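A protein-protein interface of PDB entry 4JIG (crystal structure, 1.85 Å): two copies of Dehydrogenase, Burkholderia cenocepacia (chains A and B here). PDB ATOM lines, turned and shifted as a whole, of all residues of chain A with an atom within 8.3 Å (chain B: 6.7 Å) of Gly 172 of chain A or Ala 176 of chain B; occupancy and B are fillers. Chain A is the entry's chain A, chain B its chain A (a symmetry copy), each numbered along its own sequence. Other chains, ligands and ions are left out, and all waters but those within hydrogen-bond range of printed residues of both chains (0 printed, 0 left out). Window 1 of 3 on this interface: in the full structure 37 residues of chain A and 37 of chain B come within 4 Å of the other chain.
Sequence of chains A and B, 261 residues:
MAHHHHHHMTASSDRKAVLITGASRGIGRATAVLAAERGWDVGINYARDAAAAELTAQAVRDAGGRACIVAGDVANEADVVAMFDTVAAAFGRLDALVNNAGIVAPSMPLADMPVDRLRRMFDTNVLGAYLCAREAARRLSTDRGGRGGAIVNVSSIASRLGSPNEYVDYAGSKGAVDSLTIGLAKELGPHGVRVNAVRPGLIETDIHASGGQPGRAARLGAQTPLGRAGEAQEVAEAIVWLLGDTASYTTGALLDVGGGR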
ATOM      1  N   MET A 121      16.786  -5.582 -28.607  1.00  0.00           N
ATOM      2  CA  MET A 121      17.601  -6.620 -29.204  1.00  0.00           C
ATOM      3  C   MET A 121      16.786  -7.915 -29.289  1.00  0.00           C
ATOM      4  O   MET A 121      16.756  -8.589 -30.322  1.00  0.00           O
ATOM      5  CB  MET A 121      18.871  -6.847 -28.381  1.00  0.00           C
ATOM      6  CG  MET A 121      19.882  -7.818 -28.993  1.00  0.00           C
ATOM      7  SD  MET A 121      20.649  -7.202 -30.507  1.00  0.00           S
ATOM      8  CE  MET A 121      21.797  -5.975 -29.930  1.00  0.00           C
ATOM      9  N   PHE A 122      16.169  -8.280 -28.185  1.00  0.00           N
ATOM     10  CA  PHE A 122      15.454  -9.545 -28.135  1.00  0.00           C
ATOM     11  C   PHE A 122      14.138  -9.504 -28.898  1.00  0.00           C
ATOM     12  O   PHE A 122      13.780 -10.452 -29.583  1.00  0.00           O
ATOM     13  CB  PHE A 122      15.286  -9.990 -26.687  1.00  0.00           C
ATOM     14  CG  PHE A 122      16.577 -10.159 -25.955  1.00  0.00           C
ATOM     15  CD1 PHE A 122      17.668 -10.796 -26.540  1.00  0.00           C
ATOM     16  CD2 PHE A 122      16.687  -9.731 -24.664  1.00  0.00           C
ATOM     17  CE1 PHE A 122      18.857 -10.963 -25.831  1.00  0.00           C
ATOM     18  CE2 PHE A 122      17.866  -9.860 -23.955  1.00  0.00           C
ATOM     19  CZ  PHE A 122      18.954 -10.495 -24.533  1.00  0.00           C
ATOM     20  N   ASN A 125      15.391  -9.586 -32.669  1.00  0.00           N
ATOM     21  CA  ASN A 125      16.149 -10.747 -33.127  1.00  0.00           C
ATOM     22  C   ASN A 125      15.594 -12.075 -32.693  1.00  0.00           C
ATOM     23  O   ASN A 125      15.856 -13.098 -33.349  1.00  0.00           O
ATOM     24  CB  ASN A 125      17.594 -10.644 -32.673  1.00  0.00           C
ATOM     25  CG  ASN A 125      18.396  -9.740 -33.552  1.00  0.00           C
ATOM     26  OD1 ASN A 125      18.724 -10.110 -34.680  1.00  0.00           O
ATOM     27  ND2 ASN A 125      18.755  -8.563 -33.042  1.00  0.00           N
ATOM     28  N   VAL A 126      14.833 -12.077 -31.598  1.00  0.00           N
ATOM     29  CA  VAL A 126      14.232 -13.314 -31.118  1.00  0.00           C
ATOM     30  C   VAL A 126      12.746 -13.309 -31.402  1.00  0.00           C
ATOM     31  O   VAL A 126      12.282 -14.115 -32.191  1.00  0.00           O
ATOM     32  CB  VAL A 126      14.493 -13.547 -29.610  1.00  0.00           C
ATOM     33  CG1 VAL A 126      13.881 -14.865 -29.155  1.00  0.00           C
ATOM     34  CG2 VAL A 126      15.985 -13.503 -29.309  1.00  0.00           C
ATOM     35  N   TYR A 130      10.865 -15.287 -34.537  1.00  0.00           N
ATOM     36  CA  TYR A 130       9.794 -16.266 -34.263  1.00  0.00           C
ATOM     37  C   TYR A 130       8.467 -15.892 -34.921  1.00  0.00           C
ATOM     38  O   TYR A 130       7.756 -16.763 -35.447  1.00  0.00           O
ATOM     39  CB  TYR A 130       9.598 -16.532 -32.756  1.00  0.00           C
ATOM     40  CG  TYR A 130      10.516 -17.630 -32.238  1.00  0.00           C
ATOM     41  CD1 TYR A 130      11.890 -17.389 -31.993  1.00  0.00           C
ATOM     42  CD2 TYR A 130      10.042 -18.898 -32.006  1.00  0.00           C
ATOM     43  CE1 TYR A 130      12.719 -18.405 -31.536  1.00  0.00           C
ATOM     44  CE2 TYR A 130      10.872 -19.929 -31.595  1.00  0.00           C
ATOM     45  CZ  TYR A 130      12.211 -19.688 -31.334  1.00  0.00           C
ATOM     46  OH  TYR A 130      13.017 -20.727 -30.878  1.00  0.00           O
ATOM     47  N   SER A 155      21.767 -15.750 -38.806  1.00  0.00           N
ATOM     48  CA  SER A 155      22.261 -15.820 -37.445  1.00  0.00           C
ATOM     49  C   SER A 155      23.590 -15.049 -37.436  1.00  0.00           C
ATOM     50  O   SER A 155      23.657 -13.996 -38.046  1.00  0.00           O
ATOM     51  CB  SER A 155      22.402 -17.250 -37.060  1.00  0.00           C
ATOM     52  OG  SER A 155      22.985 -17.453 -35.788  1.00  0.00           O
ATOM     53  N   ALA A 158      28.592 -14.976 -33.840  1.00  0.00           N
ATOM     54  CA  ALA A 158      28.493 -14.510 -32.461  1.00  0.00           C
ATOM     55  C   ALA A 158      27.779 -15.550 -31.585  1.00  0.00           C
ATOM     56  O   ALA A 158      28.007 -15.595 -30.393  1.00  0.00           O
ATOM     57  CB  ALA A 158      27.735 -13.191 -32.405  1.00  0.00           C
ATOM     58  N   SER A 159      26.917 -16.352 -32.177  1.00  0.00           N
ATOM     59  CA  SER A 159      26.179 -17.374 -31.394  1.00  0.00           C
ATOM     60  C   SER A 159      27.147 -18.386 -30.736  1.00  0.00           C
ATOM     61  O   SER A 159      26.875 -18.906 -29.629  1.00  0.00           O
ATOM     62  CB  SER A 159      25.136 -18.112 -32.231  1.00  0.00           C
ATOM     63  OG  SER A 159      25.714 -18.995 -33.184  1.00  0.00           O
ATOM     64  N   ARG A 160      28.241 -18.682 -31.416  1.00  0.00           N
ATOM     65  CA  ARG A 160      29.237 -19.581 -30.819  1.00  0.00           C
ATOM     66  C   ARG A 160      30.447 -18.893 -30.186  1.00  0.00           C
ATOM     67  O   ARG A 160      31.129 -19.508 -29.371  1.00  0.00           O
ATOM     68  CB  ARG A 160      29.673 -20.661 -31.775  1.00  0.00           C
ATOM     69  CG  ARG A 160      30.062 -20.212 -33.119  1.00  0.00           C
ATOM     70  CD  ARG A 160      30.566 -21.394 -33.927  1.00  0.00           C
ATOM     71  NE  ARG A 160      30.853 -20.867 -35.250  1.00  0.00           N
ATOM     72  CZ  ARG A 160      31.965 -20.214 -35.576  1.00  0.00           C
ATOM     73  NH1 ARG A 160      32.930 -20.008 -34.688  1.00  0.00           N
ATOM     74  NH2 ARG A 160      32.107 -19.742 -36.814  1.00  0.00           N
ATOM     75  N   GLY A 162      30.209 -15.519 -28.708  1.00  0.00           N
ATOM     76  CA  GLY A 162      29.700 -14.806 -27.534  1.00  0.00           C
ATOM     77  C   GLY A 162      29.785 -13.287 -27.505  1.00  0.00           C
ATOM     78  O   GLY A 162      29.176 -12.692 -26.630  1.00  0.00           O
ATOM     79  N   SER A 163      30.539 -12.676 -28.434  1.00  0.00           N
ATOM     80  CA  SER A 163      30.727 -11.198 -28.540  1.00  0.00           C
ATOM     81  C   SER A 163      30.954 -10.552 -27.199  1.00  0.00           C
ATOM     82  O   SER A 163      30.288  -9.562 -26.859  1.00  0.00           O
ATOM     83  CB  SER A 163      29.532 -10.496 -29.204  1.00  0.00           C
ATOM     84  OG  SER A 163      29.039 -11.223 -30.306  1.00  0.00           O
ATOM     85  N   TYR A 167      28.579  -7.277 -27.740  1.00  0.00           N
ATOM     86  CA  TYR A 167      27.168  -7.487 -28.022  1.00  0.00           C
ATOM     87  C   TYR A 167      26.772  -8.852 -27.498  1.00  0.00           C
ATOM     88  O   TYR A 167      26.247  -9.651 -28.247  1.00  0.00           O
ATOM     89  CB  TYR A 167      26.903  -7.426 -29.562  1.00  0.00           C
ATOM     90  CG  TYR A 167      27.512  -6.265 -30.301  1.00  0.00           C
ATOM     91  CD1 TYR A 167      26.986  -4.998 -30.151  1.00  0.00           C
ATOM     92  CD2 TYR A 167      28.606  -6.422 -31.147  1.00  0.00           C
ATOM     93  CE1 TYR A 167      27.523  -3.910 -30.795  1.00  0.00           C
ATOM     94  CE2 TYR A 167      29.161  -5.323 -31.801  1.00  0.00           C
ATOM     95  CZ  TYR A 167      28.607  -4.070 -31.613  1.00  0.00           C
ATOM     96  OH  TYR A 167      29.084  -2.924 -32.223  1.00  0.00           O
ATOM     97  N   VAL A 168      27.007  -9.168 -26.221  1.00  0.00           N
ATOM     98  CA  VAL A 168      26.628 -10.500 -25.748  1.00  0.00           C
ATOM     99  C   VAL A 168      25.087 -10.763 -25.795  1.00  0.00           C
ATOM    100  O   VAL A 168      24.607 -11.925 -25.824  1.00  0.00           O
ATOM    101  CB  VAL A 168      27.254 -10.808 -24.362  1.00  0.00           C
ATOM    102  CG1 VAL A 168      26.672  -9.933 -23.260  1.00  0.00           C
ATOM    103  CG2 VAL A 168      27.040 -12.258 -23.981  1.00  0.00           C
ATOM    104  N   ASP A 169      24.305  -9.675 -25.822  1.00  0.00           N
ATOM    105  CA  ASP A 169      22.855  -9.781 -26.017  1.00  0.00           C
ATOM    106  C   ASP A 169      22.554 -10.196 -27.460  1.00  0.00           C
ATOM    107  O   ASP A 169      21.755 -11.077 -27.704  1.00  0.00           O
ATOM    108  CB  ASP A 169      22.126  -8.500 -25.612  1.00  0.00           C
ATOM    109  CG  ASP A 169      22.658  -7.240 -26.340  1.00  0.00           C
ATOM    110  OD1 ASP A 169      23.855  -7.201 -26.752  1.00  0.00           O
ATOM    111  OD2 ASP A 169      21.848  -6.311 -26.518  1.00  0.00           O
ATOM    112  N   TYR A 170      23.228  -9.574 -28.423  1.00  0.00           N
ATOM    113  CA  TYR A 170      23.096  -9.998 -29.818  1.00  0.00           C
ATOM    114  C   TYR A 170      23.512 -11.461 -29.968  1.00  0.00           C
ATOM    115  O   TYR A 170      22.840 -12.242 -30.659  1.00  0.00           O
ATOM    116  CB  TYR A 170      23.957  -9.104 -30.713  1.00  0.00           C
ATOM    117  CG  TYR A 170      24.057  -9.509 -32.151  1.00  0.00           C
ATOM    118  CD1 TYR A 170      23.035  -9.200 -33.069  1.00  0.00           C
ATOM    119  CD2 TYR A 170      25.174 -10.184 -32.623  1.00  0.00           C
ATOM    120  CE1 TYR A 170      23.140  -9.562 -34.408  1.00  0.00           C
ATOM    121  CE2 TYR A 170      25.286 -10.536 -33.966  1.00  0.00           C
ATOM    122  CZ  TYR A 170      24.285 -10.207 -34.844  1.00  0.00           C
ATOM    123  OH  TYR A 170      24.388 -10.549 -36.176  1.00  0.00           O
ATOM    124  N   ALA A 171      24.610 -11.826 -29.316  1.00  0.00           N
ATOM    125  CA  ALA A 171      25.088 -13.228 -29.340  1.00  0.00           C
ATOM    126  C   ALA A 171      24.004 -14.196 -28.883  1.00  0.00           C
ATOM    127  O   ALA A 171      23.716 -15.213 -29.537  1.00  0.00           O
ATOM    128  CB  ALA A 171      26.381 -13.362 -28.537  1.00  0.00           C
ATOM    129  N   GLY A 172      23.348 -13.878 -27.765  1.00  0.00           N
ATOM    130  CA  GLY A 172      22.282 -14.730 -27.290  1.00  0.00           C
ATOM    131  C   GLY A 172      21.147 -14.792 -28.264  1.00  0.00           C
ATOM    132  O   GLY A 172      20.532 -15.866 -28.480  1.00  0.00           O
ATOM    133  N   SER A 173      20.794 -13.628 -28.835  1.00  0.00           N
ATOM    134  CA  SER A 173      19.676 -13.636 -29.770  1.00  0.00           C
ATOM    135  C   SER A 173      19.926 -14.592 -30.941  1.00  0.00           C
ATOM    136  O   SER A 173      18.989 -15.198 -31.472  1.00  0.00           O
ATOM    137  CB  SER A 173      19.361 -12.229 -30.254  1.00  0.00           C
ATOM    138  OG  SER A 173      20.247 -11.759 -31.252  1.00  0.00           O
ATOM    139  N   LYS A 174      21.182 -14.702 -31.364  1.00  0.00           N
ATOM    140  CA  LYS A 174      21.489 -15.568 -32.499  1.00  0.00           C
ATOM    141  C   LYS A 174      21.649 -17.012 -32.074  1.00  0.00           C
ATOM    142  O   LYS A 174      21.348 -17.944 -32.857  1.00  0.00           O
ATOM    143  CB  LYS A 174      22.710 -15.005 -33.218  1.00  0.00           C
ATOM    144  CG  LYS A 174      22.403 -13.655 -33.851  1.00  0.00           C
ATOM    145  CD  LYS A 174      21.063 -13.554 -34.567  1.00  0.00           C
ATOM    146  CE  LYS A 174      21.000 -12.271 -35.384  1.00  0.00           C
ATOM    147  NZ  LYS A 174      19.850 -12.252 -36.294  1.00  0.00           N
ATOM    148  N   GLY A 175      22.057 -17.235 -30.827  1.00  0.00           N
ATOM    149  CA  GLY A 175      21.913 -18.568 -30.265  1.00  0.00           C
ATOM    150  C   GLY A 175      20.463 -19.071 -30.332  1.00  0.00           C
ATOM    151  O   GLY A 175      20.207 -20.231 -30.645  1.00  0.00           O
ATOM    152  N   ALA A 176      19.489 -18.204 -30.041  1.00  0.00           N
ATOM    153  CA  ALA A 176      18.063 -18.558 -30.140  1.00  0.00           C
ATOM    154  C   ALA A 176      17.691 -18.897 -31.583  1.00  0.00           C
ATOM    155  O   ALA A 176      16.961 -19.856 -31.824  1.00  0.00           O
ATOM    156  CB  ALA A 176      17.177 -17.424 -29.608  1.00  0.00           C
ATOM    157  N   VAL A 177      18.242 -18.144 -32.539  1.00  0.00           N
ATOM    158  CA  VAL A 177      17.948 -18.358 -33.934  1.00  0.00           C
ATOM    159  C   VAL A 177      18.511 -19.708 -34.386  1.00  0.00           C
ATOM    160  O   VAL A 177      17.880 -20.386 -35.174  1.00  0.00           O
ATOM    161  CB  VAL A 177      18.478 -17.221 -34.836  1.00  0.00           C
ATOM    162  CG1 VAL A 177      18.420 -17.598 -36.300  1.00  0.00           C
ATOM    163  CG2 VAL A 177      17.693 -15.939 -34.573  1.00  0.00           C
ATOM    164  N   ASP A 178      19.704 -20.066 -33.914  1.00  0.00           N
ATOM    165  CA  ASP A 178      20.300 -21.359 -34.277  1.00  0.00           C
ATOM    166  C   ASP A 178      19.378 -22.490 -33.773  1.00  0.00           C
ATOM    167  O   ASP A 178      19.090 -23.412 -34.517  1.00  0.00           O
ATOM    168  CB  ASP A 178      21.682 -21.554 -33.706  1.00  0.00           C
ATOM    169  CG  ASP A 178      22.761 -20.665 -34.333  1.00  0.00           C
ATOM    170  OD1 ASP A 178      22.493 -19.903 -35.295  1.00  0.00           O
ATOM    171  OD2 ASP A 178      23.895 -20.761 -33.823  1.00  0.00           O
ATOM    172  N   SER A 179      18.885 -22.378 -32.527  1.00  0.00           N
ATOM    173  CA  SER A 179      18.033 -23.391 -31.949  1.00  0.00           C
ATOM    174  C   SER A 179      16.665 -23.462 -32.633  1.00  0.00           C
ATOM    175  O   SER A 179      16.105 -24.557 -32.893  1.00  0.00           O
ATOM    176  CB  SER A 179      17.913 -23.115 -30.428  1.00  0.00           C
ATOM    177  OG  SER A 179      19.144 -23.420 -29.767  1.00  0.00           O
ATOM    178  N   LEU A 180      16.119 -22.286 -32.957  1.00  0.00           N
ATOM    179  CA  LEU A 180      14.901 -22.204 -33.765  1.00  0.00           C
ATOM    180  C   LEU A 180      15.042 -23.000 -35.074  1.00  0.00           C
ATOM    181  O   LEU A 180      14.129 -23.731 -35.493  1.00  0.00           O
ATOM    182  CB  LEU A 180      14.611 -20.748 -34.117  1.00  0.00           C
ATOM    183  CG  LEU A 180      13.573 -20.425 -35.190  1.00  0.00           C
ATOM    184  CD1 LEU A 180      12.210 -20.915 -34.787  1.00  0.00           C
ATOM    185  CD2 LEU A 180      13.514 -18.952 -35.414  1.00  0.00           C
ATOM    186  N   ASN B 125      12.694 -16.422 -20.076  1.00  0.00           N
ATOM    187  CA  ASN B 125      13.878 -17.251 -20.283  1.00  0.00           C
ATOM    188  C   ASN B 125      15.040 -16.545 -20.924  1.00  0.00           C
ATOM    189  O   ASN B 125      16.194 -16.973 -20.753  1.00  0.00           O
ATOM    190  CB  ASN B 125      13.527 -18.474 -21.111  1.00  0.00           C
ATOM    191  CG  ASN B 125      12.887 -19.545 -20.287  1.00  0.00           C
ATOM    192  OD1 ASN B 125      13.568 -20.209 -19.504  1.00  0.00           O
ATOM    193  ND2 ASN B 125      11.586 -19.756 -20.475  1.00  0.00           N
ATOM    194  N   VAL B 126      14.755 -15.471 -21.662  1.00  0.00           N
ATOM    195  CA  VAL B 126      15.819 -14.709 -22.300  1.00  0.00           C
ATOM    196  C   VAL B 126      16.019 -13.396 -21.576  1.00  0.00           C
ATOM    197  O   VAL B 126      17.066 -13.187 -20.986  1.00  0.00           O
ATOM    198  CB  VAL B 126      15.544 -14.460 -23.803  1.00  0.00           C
ATOM    199  CG1 VAL B 126      16.694 -13.694 -24.442  1.00  0.00           C
ATOM    200  CG2 VAL B 126      15.292 -15.775 -24.529  1.00  0.00           C
ATOM    201  N   TYR B 130      19.025 -12.570 -18.826  1.00  0.00           N
ATOM    202  CA  TYR B 130      19.946 -11.438 -19.048  1.00  0.00           C
ATOM    203  C   TYR B 130      19.903 -10.407 -17.922  1.00  0.00           C
ATOM    204  O   TYR B 130      20.947  -9.878 -17.510  1.00  0.00           O
ATOM    205  CB  TYR B 130      19.737 -10.756 -20.417  1.00  0.00           C
ATOM    206  CG  TYR B 130      20.541 -11.423 -21.524  1.00  0.00           C
ATOM    207  CD1 TYR B 130      20.130 -12.651 -22.098  1.00  0.00           C
ATOM    208  CD2 TYR B 130      21.704 -10.861 -21.992  1.00  0.00           C
ATOM    209  CE1 TYR B 130      20.882 -13.256 -23.097  1.00  0.00           C
ATOM    210  CE2 TYR B 130      22.485 -11.481 -22.954  1.00  0.00           C
ATOM    211  CZ  TYR B 130      22.071 -12.670 -23.531  1.00  0.00           C
ATOM    212  OH  TYR B 130      22.848 -13.252 -24.529  1.00  0.00           O
ATOM    213  N   SER B 159      18.050 -26.953 -26.344  1.00  0.00           N
ATOM    214  CA  SER B 159      18.826 -25.971 -27.139  1.00  0.00           C
ATOM    215  C   SER B 159      19.500 -26.642 -28.360  1.00  0.00           C
ATOM    216  O   SER B 159      19.664 -26.010 -29.429  1.00  0.00           O
ATOM    217  CB  SER B 159      19.869 -25.232 -26.302  1.00  0.00           C
ATOM    218  OG  SER B 159      20.960 -26.060 -25.920  1.00  0.00           O
ATOM    219  N   ALA B 171      13.044 -23.986 -26.702  1.00  0.00           N
ATOM    220  CA  ALA B 171      14.341 -24.403 -27.286  1.00  0.00           C
ATOM    221  C   ALA B 171      15.195 -23.200 -27.664  1.00  0.00           C
ATOM    222  O   ALA B 171      16.386 -23.107 -27.319  1.00  0.00           O
ATOM    223  CB  ALA B 171      14.114 -25.361 -28.454  1.00  0.00           C
ATOM    224  N   GLY B 172      14.592 -22.227 -28.351  1.00  0.00           N
ATOM    225  CA  GLY B 172      15.330 -21.040 -28.714  1.00  0.00           C
ATOM    226  C   GLY B 172      15.784 -20.279 -27.508  1.00  0.00           C
ATOM    227  O   GLY B 172      16.914 -19.735 -27.468  1.00  0.00           O
ATOM    228  N   SER B 173      14.890 -20.166 -26.510  1.00  0.00           N
ATOM    229  CA  SER B 173      15.279 -19.411 -25.325  1.00  0.00           C
ATOM    230  C   SER B 173      16.534 -19.997 -24.669  1.00  0.00           C
ATOM    231  O   SER B 173      17.347 -19.263 -24.096  1.00  0.00           O
ATOM    232  CB  SER B 173      14.125 -19.313 -24.339  1.00  0.00           C
ATOM    233  OG  SER B 173      13.928 -20.488 -23.577  1.00  0.00           O
ATOM    234  N   LYS B 174      16.674 -21.318 -24.724  1.00  0.00           N
ATOM    235  CA  LYS B 174      17.828 -21.949 -24.089  1.00  0.00           C
ATOM    236  C   LYS B 174      19.047 -21.918 -24.985  1.00  0.00           C
ATOM    237  O   LYS B 174      20.199 -21.857 -24.494  1.00  0.00           O
ATOM    238  CB  LYS B 174      17.428 -23.353 -23.651  1.00  0.00           C
ATOM    239  CG  LYS B 174      16.376 -23.309 -22.553  1.00  0.00           C
ATOM    240  CD  LYS B 174      16.610 -22.277 -21.458  1.00  0.00           C
ATOM    241  CE  LYS B 174      15.658 -22.522 -20.294  1.00  0.00           C
ATOM    242  NZ  LYS B 174      16.016 -21.729 -19.114  1.00  0.00           N
ATOM    243  N   GLY B 175      18.833 -21.893 -26.299  1.00  0.00           N
ATOM    244  CA  GLY B 175      19.927 -21.534 -27.186  1.00  0.00           C
ATOM    245  C   GLY B 175      20.536 -20.168 -26.830  1.00  0.00           C
ATOM    246  O   GLY B 175      21.752 -19.992 -26.847  1.00  0.00           O
ATOM    247  N   ALA B 176      19.699 -19.180 -26.503  1.00  0.00           N
ATOM    248  CA  ALA B 176      20.175 -17.853 -26.078  1.00  0.00           C
ATOM    249  C   ALA B 176      20.980 -17.957 -24.784  1.00  0.00           C
ATOM    250  O   ALA B 176      22.019 -17.316 -24.649  1.00  0.00           O
ATOM    251  CB  ALA B 176      19.003 -16.878 -25.907  1.00  0.00           C
ATOM    252  N   VAL B 177      20.527 -18.811 -23.861  1.00  0.00           N
ATOM    253  CA  VAL B 177      21.193 -18.978 -22.593  1.00  0.00           C
ATOM    254  C   VAL B 177      22.568 -19.615 -22.805  1.00  0.00           C
ATOM    255  O   VAL B 177      23.508 -19.252 -22.122  1.00  0.00           O
ATOM    256  CB  VAL B 177      20.361 -19.806 -21.588  1.00  0.00           C
ATOM    257  CG1 VAL B 177      21.185 -20.213 -20.386  1.00  0.00           C
ATOM    258  CG2 VAL B 177      19.126 -19.018 -21.160  1.00  0.00           C
ATOM    259  N   ASP B 178      22.667 -20.579 -23.718  1.00  0.00           N
ATOM    260  CA  ASP B 178      23.958 -21.220 -24.001  1.00  0.00           C
ATOM    261  C   ASP B 178      24.939 -20.150 -24.525  1.00  0.00           C
ATOM    262  O   ASP B 178      26.068 -20.090 -24.069  1.00  0.00           O
ATOM    263  CB  ASP B 178      23.855 -22.337 -25.010  1.00  0.00           C
ATOM    264  CG  ASP B 178      23.130 -23.587 -24.504  1.00  0.00           C
ATOM    265  OD1 ASP B 178      22.733 -23.669 -23.314  1.00  0.00           O
ATOM    266  OD2 ASP B 178      22.972 -24.492 -25.347  1.00  0.00           O
ATOM    267  N   SER B 179      24.478 -19.284 -25.445  1.00  0.00           N
ATOM    268  CA  SER B 179      25.319 -18.260 -26.019  1.00  0.00           C
ATOM    269  C   SER B 179      25.708 -17.186 -25.000  1.00  0.00           C
ATOM    270  O   SER B 179      26.868 -16.707 -24.945  1.00  0.00           O
ATOM    271  CB  SER B 179      24.587 -17.663 -27.249  1.00  0.00           C
ATOM    272  OG  SER B 179      24.572 -18.604 -28.326  1.00  0.00           O
ATOM    273  N   LEU B 180      24.740 -16.810 -24.158  1.00  0.00           N
ATOM    274  CA  LEU B 180      25.011 -15.922 -23.026  1.00  0.00           C
ATOM    275  C   LEU B 180      26.167 -16.455 -22.161  1.00  0.00           C
ATOM    276  O   LEU B 180      27.060 -15.704 -21.735  1.00  0.00           O
ATOM    277  CB  LEU B 180      23.768 -15.807 -22.150  1.00  0.00           C
ATOM    278  CG  LEU B 180      23.881 -15.182 -20.760  1.00  0.00           C
ATOM    279  CD1 LEU B 180      24.322 -13.748 -20.848  1.00  0.00           C
ATOM    280  CD2 LEU B 180      22.563 -15.245 -20.066  1.00  0.00           C
ATOM    281  N   THR B 181      26.080 -17.743 -21.882  1.00  0.00           N
ATOM    282  CA  THR B 181      27.053 -18.427 -21.036  1.00  0.00           C
ATOM    283  C   THR B 181      28.431 -18.295 -21.612  1.00  0.00           C
ATOM    284  O   THR B 181      29.351 -17.886 -20.905  1.00  0.00           O
ATOM    285  CB  THR B 181      26.682 -19.893 -20.817  1.00  0.00           C
ATOM    286  OG1 THR B 181      25.398 -19.935 -20.188  1.00  0.00           O
ATOM    287  CG2 THR B 181      27.701 -20.582 -19.954  1.00  0.00           C
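Gly 162 of chain A touches none of the printed residues of chain B. Gly 172 of chain A touches three residues of chain B. Printed residues of chain B within 4 Å of Ser 179 of chain A: Ser 159, Ala 171, Gly 172 and Gly 175. Leu 180 of chain A touches none of the printed residues of chain B. Of the printed residues of chain A, Val 126 of chain B touches Phe 122. Of the printed residues of chain A, Ala 171 of chain B touches Ser 179 (3.5 Å). Printed residues of chain A within 4 Å of Gly 172 of chain B: Tyr 130, Ala 176 and Ser 179. Of chain A, only Gly 175 (3.7 Å), Ala 176 (3.9 Å) and Ser 179 (3.3 Å) come within 4 Å of Gly 175 of chain B. Ala 176 of chain B touches just these residues of chain A: Gly 172 (3.1 Å), Gly 175 (3.9 Å) and Ala 176 (3.7 Å). The nearest printed residue of chain B that does not touch Gly 175 of chain A is Gly 172 of chain B (4.6 Å).
Tyr 130 of chain A touches Gly 172 of chain B, and with the chains exchanged Gly 172 of chain A touches Tyr 130 of chain B. Ser 159 of chain A touches Ser 179 of chain B, and with the chains exchanged Ser 179 of chain A touches Ser 159 of chain B. Gly 172 of chain A touches Ala 176 of chain B, and with the chains exchanged Ala 176 of chain A touches Gly 172 of chain B. Gly 172 of chain A touches Ser 179 of chain B, and with the chains exchanged Ser 179 of chain A touches Gly 172 of chain B. Positions printed for both chains: 125, 126, 130, 159, 171, 172, 173, 174, 175, 176, 177, 178, 179 and 180. Of the 20 pairs that touch across the chains among the printed residues, 16 have their exchanged pair printed and touching as well.
N of Gly 172 of chain A lies close to OH of Tyr 130 of chain B (3.3 Å). O of Ser 159 of chain A sits at hydrogen-bond distance from OG of Ser 179 of chain B (2.7 Å). OH of Tyr 130 of chain B sits at hydrogen-bond distance from O of Val 168 of chain A, 2.6 Å away. The backbone NH of Gly 172 of chain B sits close to the side-chain hydroxyl of Tyr 130 of chain A, 3.3 Å away. The side-chain hydroxyl (OG) of Ser 179 of chain A sits at hydrogen-bond distance from the backbone carbonyl oxygen (O) of Ser 159 of chain B, 2.7 Å away.
Phe 122 of chain A touches Val 126 of chain B (CD1 to CG1, 3.7 Å). Phe 122 of chain A touches Tyr 130 of chain B (CZ to CD1, 3.5 Å). Asp 169 of chain A touches Tyr 130 of chain B. O of Gly 172 of chain A touches CA of Ala 176 of chain B, at 3.1 Å. Gly 175 of chain A touches Gly 175 of chain B. Gly 175 of chain A touches Ala 176 of chain B (C to N, 3.9 Å). CA of Gly 175 of chain A touches OG of Ser 179 of chain B, 3.3 Å away. Ala 176 of chain A touches Ala 176 of chain B. CB of Ser 179 of chain A touches O of Ala 171 of chain B (3.5 Å). Ser 179 of chain A touches Gly 172 of chain B.
Of the 15 printed residues of chain B, 8 touch a printed residue of chain A. Of the 25 printed residues of chain A, 10 touch a printed residue of chain B. Printed residues of chain A that touch a printed residue of chain B: Phe 122, Tyr 130, Ser 159, Val 168, Asp 169, Ala 171, Gly 172, Gly 175, Ala 176 and Ser 179. Hydrophobic or aromatic side chains of chain A that line the printed part of chain B: Phe 122, Tyr 130 and Ala 176.
The side-chain hydroxyl of Ser 179 of chain B is in hydrogen-bond range of the backbone carbonyl oxygen of Gly 175 of chain B (3.5 Å). N of Val 168 of chain A lies within hydrogen-bond range of O of Ser 163 of chain A (3.4 Å). OG of Ser 159 of chain B sits at hydrogen-bond distance from OD2 of Asp 178 of chain B (2.6 Å). OD2 of Asp 178 of chain A sits at hydrogen-bond distance from OG of Ser 159 of chain A, at 2.6 Å. OG of Ser 179 of chain A lies within hydrogen-bond range of O of Gly 175 of chain A (3.5 Å).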
